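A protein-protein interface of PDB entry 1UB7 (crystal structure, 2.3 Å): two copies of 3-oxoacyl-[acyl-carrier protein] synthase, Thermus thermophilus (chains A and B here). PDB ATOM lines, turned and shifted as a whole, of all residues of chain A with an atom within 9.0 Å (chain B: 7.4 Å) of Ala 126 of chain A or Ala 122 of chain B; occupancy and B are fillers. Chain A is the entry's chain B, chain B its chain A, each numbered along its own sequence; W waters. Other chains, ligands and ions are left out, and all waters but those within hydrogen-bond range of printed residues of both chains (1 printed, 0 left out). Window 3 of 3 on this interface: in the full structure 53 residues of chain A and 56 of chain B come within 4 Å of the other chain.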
ATOM      1  N   SER A   2       2.064 -27.393   6.615  1.00  0.00           N
ATOM      2  CA  SER A   2       1.856 -28.799   7.084  1.00  0.00           C
ATOM      3  C   SER A   2       1.390 -29.649   5.912  1.00  0.00           C
ATOM      4  O   SER A   2       0.943 -29.121   4.880  1.00  0.00           O
ATOM      5  CB  SER A   2       0.769 -28.852   8.153  1.00  0.00           C
ATOM      6  OG  SER A   2      -0.494 -28.591   7.545  1.00  0.00           O
ATOM      7  N   PHE A 102      -4.859 -33.360  23.426  1.00  0.00           N
ATOM      8  CA  PHE A 102      -6.176 -32.803  23.651  1.00  0.00           C
ATOM      9  C   PHE A 102      -7.060 -33.324  22.512  1.00  0.00           C
ATOM     10  O   PHE A 102      -6.557 -33.704  21.429  1.00  0.00           O
ATOM     11  CB  PHE A 102      -6.159 -31.263  23.706  1.00  0.00           C
ATOM     12  CG  PHE A 102      -5.505 -30.588  22.528  1.00  0.00           C
ATOM     13  CD1 PHE A 102      -4.128 -30.384  22.500  1.00  0.00           C
ATOM     14  CD2 PHE A 102      -6.285 -30.055  21.496  1.00  0.00           C
ATOM     15  CE1 PHE A 102      -3.530 -29.654  21.466  1.00  0.00           C
ATOM     16  CE2 PHE A 102      -5.697 -29.322  20.456  1.00  0.00           C
ATOM     17  CZ  PHE A 102      -4.321 -29.119  20.442  1.00  0.00           C
ATOM     18  N   TYR A 104     -11.263 -33.242  20.541  1.00  0.00           N
ATOM     19  CA  TYR A 104     -12.597 -32.700  20.345  1.00  0.00           C
ATOM     20  C   TYR A 104     -13.251 -33.139  19.035  1.00  0.00           C
ATOM     21  O   TYR A 104     -12.584 -33.484  18.045  1.00  0.00           O
ATOM     22  CB  TYR A 104     -12.570 -31.157  20.451  1.00  0.00           C
ATOM     23  CG  TYR A 104     -11.978 -30.400  19.281  1.00  0.00           C
ATOM     24  CD1 TYR A 104     -12.751 -30.084  18.164  1.00  0.00           C
ATOM     25  CD2 TYR A 104     -10.662 -29.948  19.313  1.00  0.00           C
ATOM     26  CE1 TYR A 104     -12.228 -29.325  17.113  1.00  0.00           C
ATOM     27  CE2 TYR A 104     -10.124 -29.196  18.257  1.00  0.00           C
ATOM     28  CZ  TYR A 104     -10.918 -28.886  17.168  1.00  0.00           C
ATOM     29  OH  TYR A 104     -10.412 -28.116  16.151  1.00  0.00           O
ATOM     30  N   ALA A 118      -7.930 -28.286   7.887  1.00  0.00           N
ATOM     31  CA  ALA A 118      -7.602 -26.864   8.036  1.00  0.00           C
ATOM     32  C   ALA A 118      -7.325 -26.463   9.507  1.00  0.00           C
ATOM     33  O   ALA A 118      -6.341 -25.776   9.776  1.00  0.00           O
ATOM     34  CB  ALA A 118      -8.743 -25.988   7.442  1.00  0.00           C
ATOM     35  N   GLN A 119      -8.178 -26.869  10.455  1.00  0.00           N
ATOM     36  CA  GLN A 119      -7.924 -26.545  11.869  1.00  0.00           C
ATOM     37  C   GLN A 119      -6.598 -27.182  12.287  1.00  0.00           C
ATOM     38  O   GLN A 119      -5.806 -26.572  13.015  1.00  0.00           O
ATOM     39  CB  GLN A 119      -8.999 -27.119  12.814  1.00  0.00           C
ATOM     40  CG  GLN A 119     -10.406 -26.743  12.482  1.00  0.00           C
ATOM     41  CD  GLN A 119     -10.603 -25.235  12.402  1.00  0.00           C
ATOM     42  OE1 GLN A 119     -10.230 -24.484  13.322  1.00  0.00           O
ATOM     43  NE2 GLN A 119     -11.197 -24.785  11.297  1.00  0.00           N
ATOM     44  N   ALA A 120      -6.384 -28.427  11.837  1.00  0.00           N
ATOM     45  CA  ALA A 120      -5.175 -29.189  12.155  1.00  0.00           C
ATOM     46  C   ALA A 120      -3.949 -28.462  11.624  1.00  0.00           C
ATOM     47  O   ALA A 120      -2.961 -28.300  12.325  1.00  0.00           O
ATOM     48  CB  ALA A 120      -5.262 -30.589  11.535  1.00  0.00           C
ATOM     49  N   HIS A 121      -4.032 -28.032  10.369  1.00  0.00           N
ATOM     50  CA  HIS A 121      -2.947 -27.320   9.727  1.00  0.00           C
ATOM     51  C   HIS A 121      -2.629 -26.098  10.572  1.00  0.00           C
ATOM     52  O   HIS A 121      -1.468 -25.774  10.788  1.00  0.00           O
ATOM     53  CB  HIS A 121      -3.361 -26.907   8.312  1.00  0.00           C
ATOM     54  CG  HIS A 121      -2.532 -25.802   7.745  1.00  0.00           C
ATOM     55  ND1 HIS A 121      -1.293 -26.012   7.176  1.00  0.00           N
ATOM     56  CD2 HIS A 121      -2.747 -24.466   7.699  1.00  0.00           C
ATOM     57  CE1 HIS A 121      -0.785 -24.852   6.803  1.00  0.00           C
ATOM     58  NE2 HIS A 121      -1.647 -23.899   7.109  1.00  0.00           N
ATOM     59  N   ALA A 122      -3.671 -25.432  11.056  1.00  0.00           N
ATOM     60  CA  ALA A 122      -3.528 -24.242  11.897  1.00  0.00           C
ATOM     61  C   ALA A 122      -2.844 -24.546  13.233  1.00  0.00           C
ATOM     62  O   ALA A 122      -1.969 -23.791  13.664  1.00  0.00           O
ATOM     63  CB  ALA A 122      -4.894 -23.621  12.150  1.00  0.00           C
ATOM     64  N   LEU A 123      -3.245 -25.633  13.893  1.00  0.00           N
ATOM     65  CA  LEU A 123      -2.629 -26.020  15.171  1.00  0.00           C
ATOM     66  C   LEU A 123      -1.135 -26.316  14.983  1.00  0.00           C
ATOM     67  O   LEU A 123      -0.308 -26.008  15.847  1.00  0.00           O
ATOM     68  CB  LEU A 123      -3.325 -27.260  15.760  1.00  0.00           C
ATOM     69  CG  LEU A 123      -4.786 -27.046  16.206  1.00  0.00           C
ATOM     70  CD1 LEU A 123      -5.423 -28.381  16.563  1.00  0.00           C
ATOM     71  CD2 LEU A 123      -4.827 -26.111  17.384  1.00  0.00           C
ATOM     72  N   VAL A 124      -0.793 -26.919  13.850  1.00  0.00           N
ATOM     73  CA  VAL A 124       0.591 -27.238  13.560  1.00  0.00           C
ATOM     74  C   VAL A 124       1.395 -25.970  13.305  1.00  0.00           C
ATOM     75  O   VAL A 124       2.397 -25.727  13.969  1.00  0.00           O
ATOM     76  CB  VAL A 124       0.689 -28.175  12.340  1.00  0.00           C
ATOM     77  CG1 VAL A 124       2.167 -28.449  11.986  1.00  0.00           C
ATOM     78  CG2 VAL A 124      -0.038 -29.478  12.663  1.00  0.00           C
ATOM     79  N   GLU A 125       0.947 -25.156  12.358  1.00  0.00           N
ATOM     80  CA  GLU A 125       1.638 -23.913  12.017  1.00  0.00           C
ATOM     81  C   GLU A 125       1.720 -22.916  13.164  1.00  0.00           C
ATOM     82  O   GLU A 125       2.684 -22.152  13.270  1.00  0.00           O
ATOM     83  CB  GLU A 125       0.945 -23.235  10.843  1.00  0.00           C
ATOM     84  CG  GLU A 125       0.976 -24.028   9.558  1.00  0.00           C
ATOM     85  CD  GLU A 125       2.388 -24.321   9.092  1.00  0.00           C
ATOM     86  OE1 GLU A 125       3.194 -23.360   9.046  1.00  0.00           O
ATOM     87  OE2 GLU A 125       2.675 -25.503   8.766  1.00  0.00           O
ATOM     88  N   ALA A 126       0.696 -22.903  14.012  1.00  0.00           N
ATOM     89  CA  ALA A 126       0.675 -21.985  15.138  1.00  0.00           C
ATOM     90  C   ALA A 126       1.463 -22.527  16.332  1.00  0.00           C
ATOM     91  O   ALA A 126       1.625 -21.836  17.340  1.00  0.00           O
ATOM     92  CB  ALA A 126      -0.759 -21.685  15.542  1.00  0.00           C
ATOM     93  N   GLY A 127       1.933 -23.766  16.226  1.00  0.00           N
ATOM     94  CA  GLY A 127       2.716 -24.354  17.297  1.00  0.00           C
ATOM     95  C   GLY A 127       1.967 -24.882  18.506  1.00  0.00           C
ATOM     96  O   GLY A 127       2.570 -25.052  19.566  1.00  0.00           O
ATOM     97  N   LEU A 128       0.667 -25.135  18.382  1.00  0.00           N
ATOM     98  CA  LEU A 128      -0.096 -25.677  19.513  1.00  0.00           C
ATOM     99  C   LEU A 128      -0.074 -27.190  19.455  1.00  0.00           C
ATOM    100  O   LEU A 128      -0.460 -27.861  20.408  1.00  0.00           O
ATOM    101  CB  LEU A 128      -1.548 -25.198  19.471  1.00  0.00           C
ATOM    102  CG  LEU A 128      -1.757 -23.683  19.501  1.00  0.00           C
ATOM    103  CD1 LEU A 128      -3.235 -23.369  19.679  1.00  0.00           C
ATOM    104  CD2 LEU A 128      -0.971 -23.093  20.636  1.00  0.00           C
ATOM    105  N   ALA A 129       0.368 -27.734  18.325  1.00  0.00           N
ATOM    106  CA  ALA A 129       0.445 -29.176  18.163  1.00  0.00           C
ATOM    107  C   ALA A 129       1.572 -29.524  17.210  1.00  0.00           C
ATOM    108  O   ALA A 129       1.776 -28.846  16.210  1.00  0.00           O
ATOM    109  CB  ALA A 129      -0.888 -29.721  17.625  1.00  0.00           C
ATOM    110  N   GLN A 130       2.320 -30.573  17.524  1.00  0.00           N
ATOM    111  CA  GLN A 130       3.400 -30.986  16.647  1.00  0.00           C
ATOM    112  C   GLN A 130       2.753 -31.748  15.484  1.00  0.00           C
ATOM    113  O   GLN A 130       3.085 -31.527  14.317  1.00  0.00           O
ATOM    114  CB  GLN A 130       4.391 -31.887  17.387  1.00  0.00           C
ATOM    115  CG  GLN A 130       5.546 -32.333  16.495  1.00  0.00           C
ATOM    116  CD  GLN A 130       6.348 -33.496  17.063  1.00  0.00           C
ATOM    117  OE1 GLN A 130       7.076 -34.159  16.330  1.00  0.00           O
ATOM    118  NE2 GLN A 130       6.218 -33.749  18.364  1.00  0.00           N
ATOM    119  N   SER B   2      -2.382 -13.531  19.105  1.00  0.00           N
ATOM    120  CA  SER B   2      -3.783 -13.025  19.027  1.00  0.00           C
ATOM    121  C   SER B   2      -4.308 -12.728  20.421  1.00  0.00           C
ATOM    122  O   SER B   2      -3.685 -13.086  21.424  1.00  0.00           O
ATOM    123  CB  SER B   2      -4.690 -14.061  18.356  1.00  0.00           C
ATOM    124  OG  SER B   2      -4.989 -15.129  19.237  1.00  0.00           O
ATOM    125  N   ALA B 116     -11.901 -23.688  22.077  1.00  0.00           N
ATOM    126  CA  ALA B 116     -12.233 -22.821  20.937  1.00  0.00           C
ATOM    127  C   ALA B 116     -11.317 -21.594  20.839  1.00  0.00           C
ATOM    128  O   ALA B 116     -11.009 -21.124  19.740  1.00  0.00           O
ATOM    129  CB  ALA B 116     -13.689 -22.367  21.022  1.00  0.00           C
ATOM    130  N   LEU B 117     -10.901 -21.067  21.987  1.00  0.00           N
ATOM    131  CA  LEU B 117     -10.033 -19.898  21.999  1.00  0.00           C
ATOM    132  C   LEU B 117      -8.689 -20.293  21.417  1.00  0.00           C
ATOM    133  O   LEU B 117      -8.102 -19.545  20.632  1.00  0.00           O
ATOM    134  CB  LEU B 117      -9.856 -19.344  23.433  1.00  0.00           C
ATOM    135  CG  LEU B 117     -11.086 -18.704  24.112  1.00  0.00           C
ATOM    136  CD1 LEU B 117     -10.751 -18.310  25.544  1.00  0.00           C
ATOM    137  CD2 LEU B 117     -11.540 -17.473  23.320  1.00  0.00           C
ATOM    138  N   ALA B 118      -8.211 -21.477  21.800  1.00  0.00           N
ATOM    139  CA  ALA B 118      -6.934 -21.969  21.308  1.00  0.00           C
ATOM    140  C   ALA B 118      -7.049 -22.183  19.806  1.00  0.00           C
ATOM    141  O   ALA B 118      -6.172 -21.771  19.035  1.00  0.00           O
ATOM    142  CB  ALA B 118      -6.565 -23.268  22.005  1.00  0.00           C
ATOM    143  N   GLN B 119      -8.138 -22.813  19.381  1.00  0.00           N
ATOM    144  CA  GLN B 119      -8.341 -23.042  17.951  1.00  0.00           C
ATOM    145  C   GLN B 119      -8.449 -21.725  17.181  1.00  0.00           C
ATOM    146  O   GLN B 119      -7.947 -21.603  16.053  1.00  0.00           O
ATOM    147  CB  GLN B 119      -9.597 -23.884  17.711  1.00  0.00           C
ATOM    148  CG  GLN B 119      -9.310 -25.358  17.473  1.00  0.00           C
ATOM    149  CD  GLN B 119      -8.562 -25.637  16.157  1.00  0.00           C
ATOM    150  OE1 GLN B 119      -8.081 -26.746  15.956  1.00  0.00           O
ATOM    151  NE2 GLN B 119      -8.476 -24.639  15.262  1.00  0.00           N
ATOM    152  N   ALA B 120      -9.107 -20.743  17.793  1.00  0.00           N
ATOM    153  CA  ALA B 120      -9.271 -19.440  17.172  1.00  0.00           C
ATOM    154  C   ALA B 120      -7.907 -18.799  17.024  1.00  0.00           C
ATOM    155  O   ALA B 120      -7.575 -18.246  15.967  1.00  0.00           O
ATOM    156  CB  ALA B 120     -10.155 -18.582  18.006  1.00  0.00           C
ATOM    157  N   HIS B 121      -7.119 -18.894  18.087  1.00  0.00           N
ATOM    158  CA  HIS B 121      -5.762 -18.362  18.101  1.00  0.00           C
ATOM    159  C   HIS B 121      -4.962 -18.940  16.915  1.00  0.00           C
ATOM    160  O   HIS B 121      -4.354 -18.192  16.135  1.00  0.00           O
ATOM    161  CB  HIS B 121      -5.083 -18.737  19.423  1.00  0.00           C
ATOM    162  CG  HIS B 121      -3.608 -18.458  19.451  1.00  0.00           C
ATOM    163  ND1 HIS B 121      -3.089 -17.185  19.568  1.00  0.00           N
ATOM    164  CD2 HIS B 121      -2.541 -19.290  19.361  1.00  0.00           C
ATOM    165  CE1 HIS B 121      -1.768 -17.245  19.546  1.00  0.00           C
ATOM    166  NE2 HIS B 121      -1.409 -18.511  19.419  1.00  0.00           N
ATOM    167  N   ALA B 122      -4.973 -20.267  16.784  1.00  0.00           N
ATOM    168  CA  ALA B 122      -4.248 -20.952  15.714  1.00  0.00           C
ATOM    169  C   ALA B 122      -4.695 -20.459  14.347  1.00  0.00           C
ATOM    170  O   ALA B 122      -3.865 -20.175  13.479  1.00  0.00           O
ATOM    171  CB  ALA B 122      -4.460 -22.433  15.820  1.00  0.00           C
ATOM    172  N   LEU B 123      -6.009 -20.363  14.157  1.00  0.00           N
ATOM    173  CA  LEU B 123      -6.571 -19.869  12.905  1.00  0.00           C
ATOM    174  C   LEU B 123      -6.057 -18.465  12.565  1.00  0.00           C
ATOM    175  O   LEU B 123      -5.643 -18.205  11.434  1.00  0.00           O
ATOM    176  CB  LEU B 123      -8.099 -19.825  12.980  1.00  0.00           C
ATOM    177  CG  LEU B 123      -8.863 -21.140  13.100  1.00  0.00           C
ATOM    178  CD1 LEU B 123     -10.384 -20.854  13.097  1.00  0.00           C
ATOM    179  CD2 LEU B 123      -8.487 -22.067  11.932  1.00  0.00           C
ATOM    180  N   VAL B 124      -6.102 -17.554  13.535  1.00  0.00           N
ATOM    181  CA  VAL B 124      -5.627 -16.188  13.307  1.00  0.00           C
ATOM    182  C   VAL B 124      -4.111 -16.167  13.025  1.00  0.00           C
ATOM    183  O   VAL B 124      -3.653 -15.515  12.086  1.00  0.00           O
ATOM    184  CB  VAL B 124      -5.914 -15.285  14.524  1.00  0.00           C
ATOM    185  CG1 VAL B 124      -5.289 -13.905  14.309  1.00  0.00           C
ATOM    186  CG2 VAL B 124      -7.410 -15.163  14.743  1.00  0.00           C
ATOM    187  N   GLU B 125      -3.352 -16.889  13.846  1.00  0.00           N
ATOM    188  CA  GLU B 125      -1.913 -16.958  13.708  1.00  0.00           C
ATOM    189  C   GLU B 125      -1.446 -17.632  12.425  1.00  0.00           C
ATOM    190  O   GLU B 125      -0.415 -17.235  11.874  1.00  0.00           O
ATOM    191  CB  GLU B 125      -1.300 -17.673  14.916  1.00  0.00           C
ATOM    192  CG  GLU B 125      -1.471 -16.928  16.240  1.00  0.00           C
ATOM    193  CD  GLU B 125      -0.892 -15.523  16.191  1.00  0.00           C
ATOM    194  OE1 GLU B 125       0.269 -15.393  15.754  1.00  0.00           O
ATOM    195  OE2 GLU B 125      -1.590 -14.559  16.583  1.00  0.00           O
ATOM    196  N   ALA B 126      -2.186 -18.640  11.952  1.00  0.00           N
ATOM    197  CA  ALA B 126      -1.807 -19.341  10.726  1.00  0.00           C
ATOM    198  C   ALA B 126      -2.366 -18.586   9.544  1.00  0.00           C
ATOM    199  O   ALA B 126      -2.170 -18.966   8.394  1.00  0.00           O
ATOM    200  CB  ALA B 126      -2.330 -20.775  10.727  1.00  0.00           C
ATOM    201  N   GLY B 127      -3.076 -17.508   9.835  1.00  0.00           N
ATOM    202  CA  GLY B 127      -3.625 -16.710   8.768  1.00  0.00           C
ATOM    203  C   GLY B 127      -4.819 -17.296   8.059  1.00  0.00           C
ATOM    204  O   GLY B 127      -5.146 -16.848   6.955  1.00  0.00           O
ATOM    205  N   LEU B 128      -5.494 -18.280   8.650  1.00  0.00           N
ATOM    206  CA  LEU B 128      -6.662 -18.840   7.957  1.00  0.00           C
ATOM    207  C   LEU B 128      -7.887 -17.970   8.214  1.00  0.00           C
ATOM    208  O   LEU B 128      -8.867 -18.043   7.485  1.00  0.00           O
ATOM    209  CB  LEU B 128      -6.940 -20.279   8.400  1.00  0.00           C
ATOM    210  CG  LEU B 128      -5.869 -21.336   8.091  1.00  0.00           C
ATOM    211  CD1 LEU B 128      -6.405 -22.698   8.471  1.00  0.00           C
ATOM    212  CD2 LEU B 128      -5.495 -21.318   6.618  1.00  0.00           C
ATOM    213  N   ALA B 129      -7.829 -17.154   9.261  1.00  0.00           N
ATOM    214  CA  ALA B 129      -8.934 -16.250   9.588  1.00  0.00           C
ATOM    215  C   ALA B 129      -8.342 -14.981  10.162  1.00  0.00           C
ATOM    216  O   ALA B 129      -7.332 -15.038  10.855  1.00  0.00           O
ATOM    217  CB  ALA B 129      -9.861 -16.879  10.611  1.00  0.00           C
ATOM    218  N   VAL B 132     -11.955 -14.382  14.669  1.00  0.00           N
ATOM    219  CA  VAL B 132     -12.813 -15.528  14.882  1.00  0.00           C
ATOM    220  C   VAL B 132     -13.802 -15.252  15.989  1.00  0.00           C
ATOM    221  O   VAL B 132     -13.422 -14.733  17.029  1.00  0.00           O
ATOM    222  CB  VAL B 132     -11.990 -16.783  15.302  1.00  0.00           C
ATOM    223  CG1 VAL B 132     -12.925 -17.966  15.533  1.00  0.00           C
ATOM    224  CG2 VAL B 132     -10.997 -17.130  14.233  1.00  0.00           C
ATOM    225  N   VAL B 164     -11.780 -13.219  18.598  1.00  0.00           N
ATOM    226  CA  VAL B 164     -10.337 -13.355  18.731  1.00  0.00           C
ATOM    227  C   VAL B 164      -9.677 -12.767  17.480  1.00  0.00           C
ATOM    228  O   VAL B 164     -10.105 -13.038  16.351  1.00  0.00           O
ATOM    229  CB  VAL B 164      -9.931 -14.842  18.917  1.00  0.00           C
ATOM    230  CG1 VAL B 164      -8.431 -14.975  18.929  1.00  0.00           C
ATOM    231  CG2 VAL B 164     -10.512 -15.374  20.222  1.00  0.00           C
ATOM    232  N   PHE B 176      -1.340 -21.844  26.365  1.00  0.00           N
ATOM    233  CA  PHE B 176      -2.507 -22.716  26.355  1.00  0.00           C
ATOM    234  C   PHE B 176      -2.029 -24.078  26.841  1.00  0.00           C
ATOM    235  O   PHE B 176      -0.953 -24.546  26.456  1.00  0.00           O
ATOM    236  CB  PHE B 176      -3.074 -22.915  24.931  1.00  0.00           C
ATOM    237  CG  PHE B 176      -3.809 -21.723  24.364  1.00  0.00           C
ATOM    238  CD1 PHE B 176      -5.116 -21.441  24.758  1.00  0.00           C
ATOM    239  CD2 PHE B 176      -3.192 -20.900  23.410  1.00  0.00           C
ATOM    240  CE1 PHE B 176      -5.812 -20.346  24.209  1.00  0.00           C
ATOM    241  CE2 PHE B 176      -3.867 -19.801  22.851  1.00  0.00           C
ATOM    242  CZ  PHE B 176      -5.183 -19.521  23.252  1.00  0.00           C
HETATM  243  O   HOH W   1       1.020 -19.727  19.053  1.00  0.00           O
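Water W1 bridges NE2 of His 121 of chain B (2.7 Å) and O of Ala 126 of chain A (2.8 Å).
Printed residues of chain A that touch a printed residue of chain B: Tyr 104, Ala 118, Gln 119, Ala 122, Leu 123, Ala 126 and Leu 128.
Among the printed residues, 11 pairs touch across the chains.
O of Leu 123 of chain B lies within hydrogen-bond range of N of Leu 128 of chain B, at 2.8 Å.
O of Leu 123 of chain A lies within hydrogen-bond range of N of Ala 129 of chain A (3.1 Å).
N of Ala 129 of chain B sits at hydrogen-bond distance from O of Leu 123 of chain B, 3.3 Å away.
O of Leu 123 of chain A sits at hydrogen-bond distance from N of Leu 128 of chain A (2.9 Å).
Among the printed residues, pairs that only touch across the chains: Ala 118 of chain A with Leu 128 of chain B (3.3 Å), Gln 119 of chain A with Leu 123 of chain B (3.3 Å), Ala 122 of chain A with Ala 122 of chain B (3.6 Å), Ala 122 of chain A with Leu 123 of chain B (3.9 Å), Ala 122 of chain A with Ala 126 of chain B (3.9 Å), Leu 123 of chain A with Gln 119 of chain B (3.2 Å), Leu 123 of chain A with Ala 122 of chain B (3.9 Å), Ala 126 of chain A with Ala 122 of chain B (3.6 Å) and Leu 128 of chain A with Ala 118 of chain B (3.4 Å).
The side-chain amide oxygen (OE1) of Gln 119 of chain B sits at hydrogen-bond distance from the side-chain hydroxyl (OH) of Tyr 104 of chain A, 2.7 Å away.
The side-chain amide nitrogen (NE2) of Gln 119 of chain B is in hydrogen-bond range of the side-chain amide oxygen (OE1) of Gln 119 of chain A.
Phe 102 of chain A touches none of the printed residues of chain B.
Printed residues of chain B within 4 Å of Ala 118 of chain A: Leu 128 (3.3 Å).
Printed residues of chain B within 4 Å of Gln 119 of chain A: Gln 119 (2.6 Å) and Leu 123 (3.3 Å).
Of the printed residues of chain B, Ala 122 of chain A touches Ala 122, Leu 123 and Ala 126.
Ala 126 of chain A touches one residue of chain B.
Gln 130 of chain A touches none of the printed residues of chain B.
Of chain A, only Ala 122 (3.6 Å), Leu 123 (3.9 Å) and Ala 126 (3.6 Å) come within 4 Å of Ala 122 of chain B.
Printed residues of chain A within 4 Å of Leu 123 of chain B: Gln 119 and Ala 122.
The nearest residue of chain B that does not touch Ala 126 of chain A is Glu 125 of chain B (4.1 Å).
Ala 118 of chain A touches Leu 128 of chain B, and with the chains exchanged Leu 128 of chain A touches Ala 118 of chain B.
Gln 119 of chain B touches its own counterpart, Gln 119 of chain A.
Ala 122 of chain A touches its own counterpart, Ala 122 of chain B.
Ala 122 of chain A touches Leu 123 of chain B, and with the chains exchanged Leu 123 of chain A touches Ala 122 of chain B.
Of the 11 pairs that touch across the chains among the printed residues, 10 have their exchanged pair printed and touching as well.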
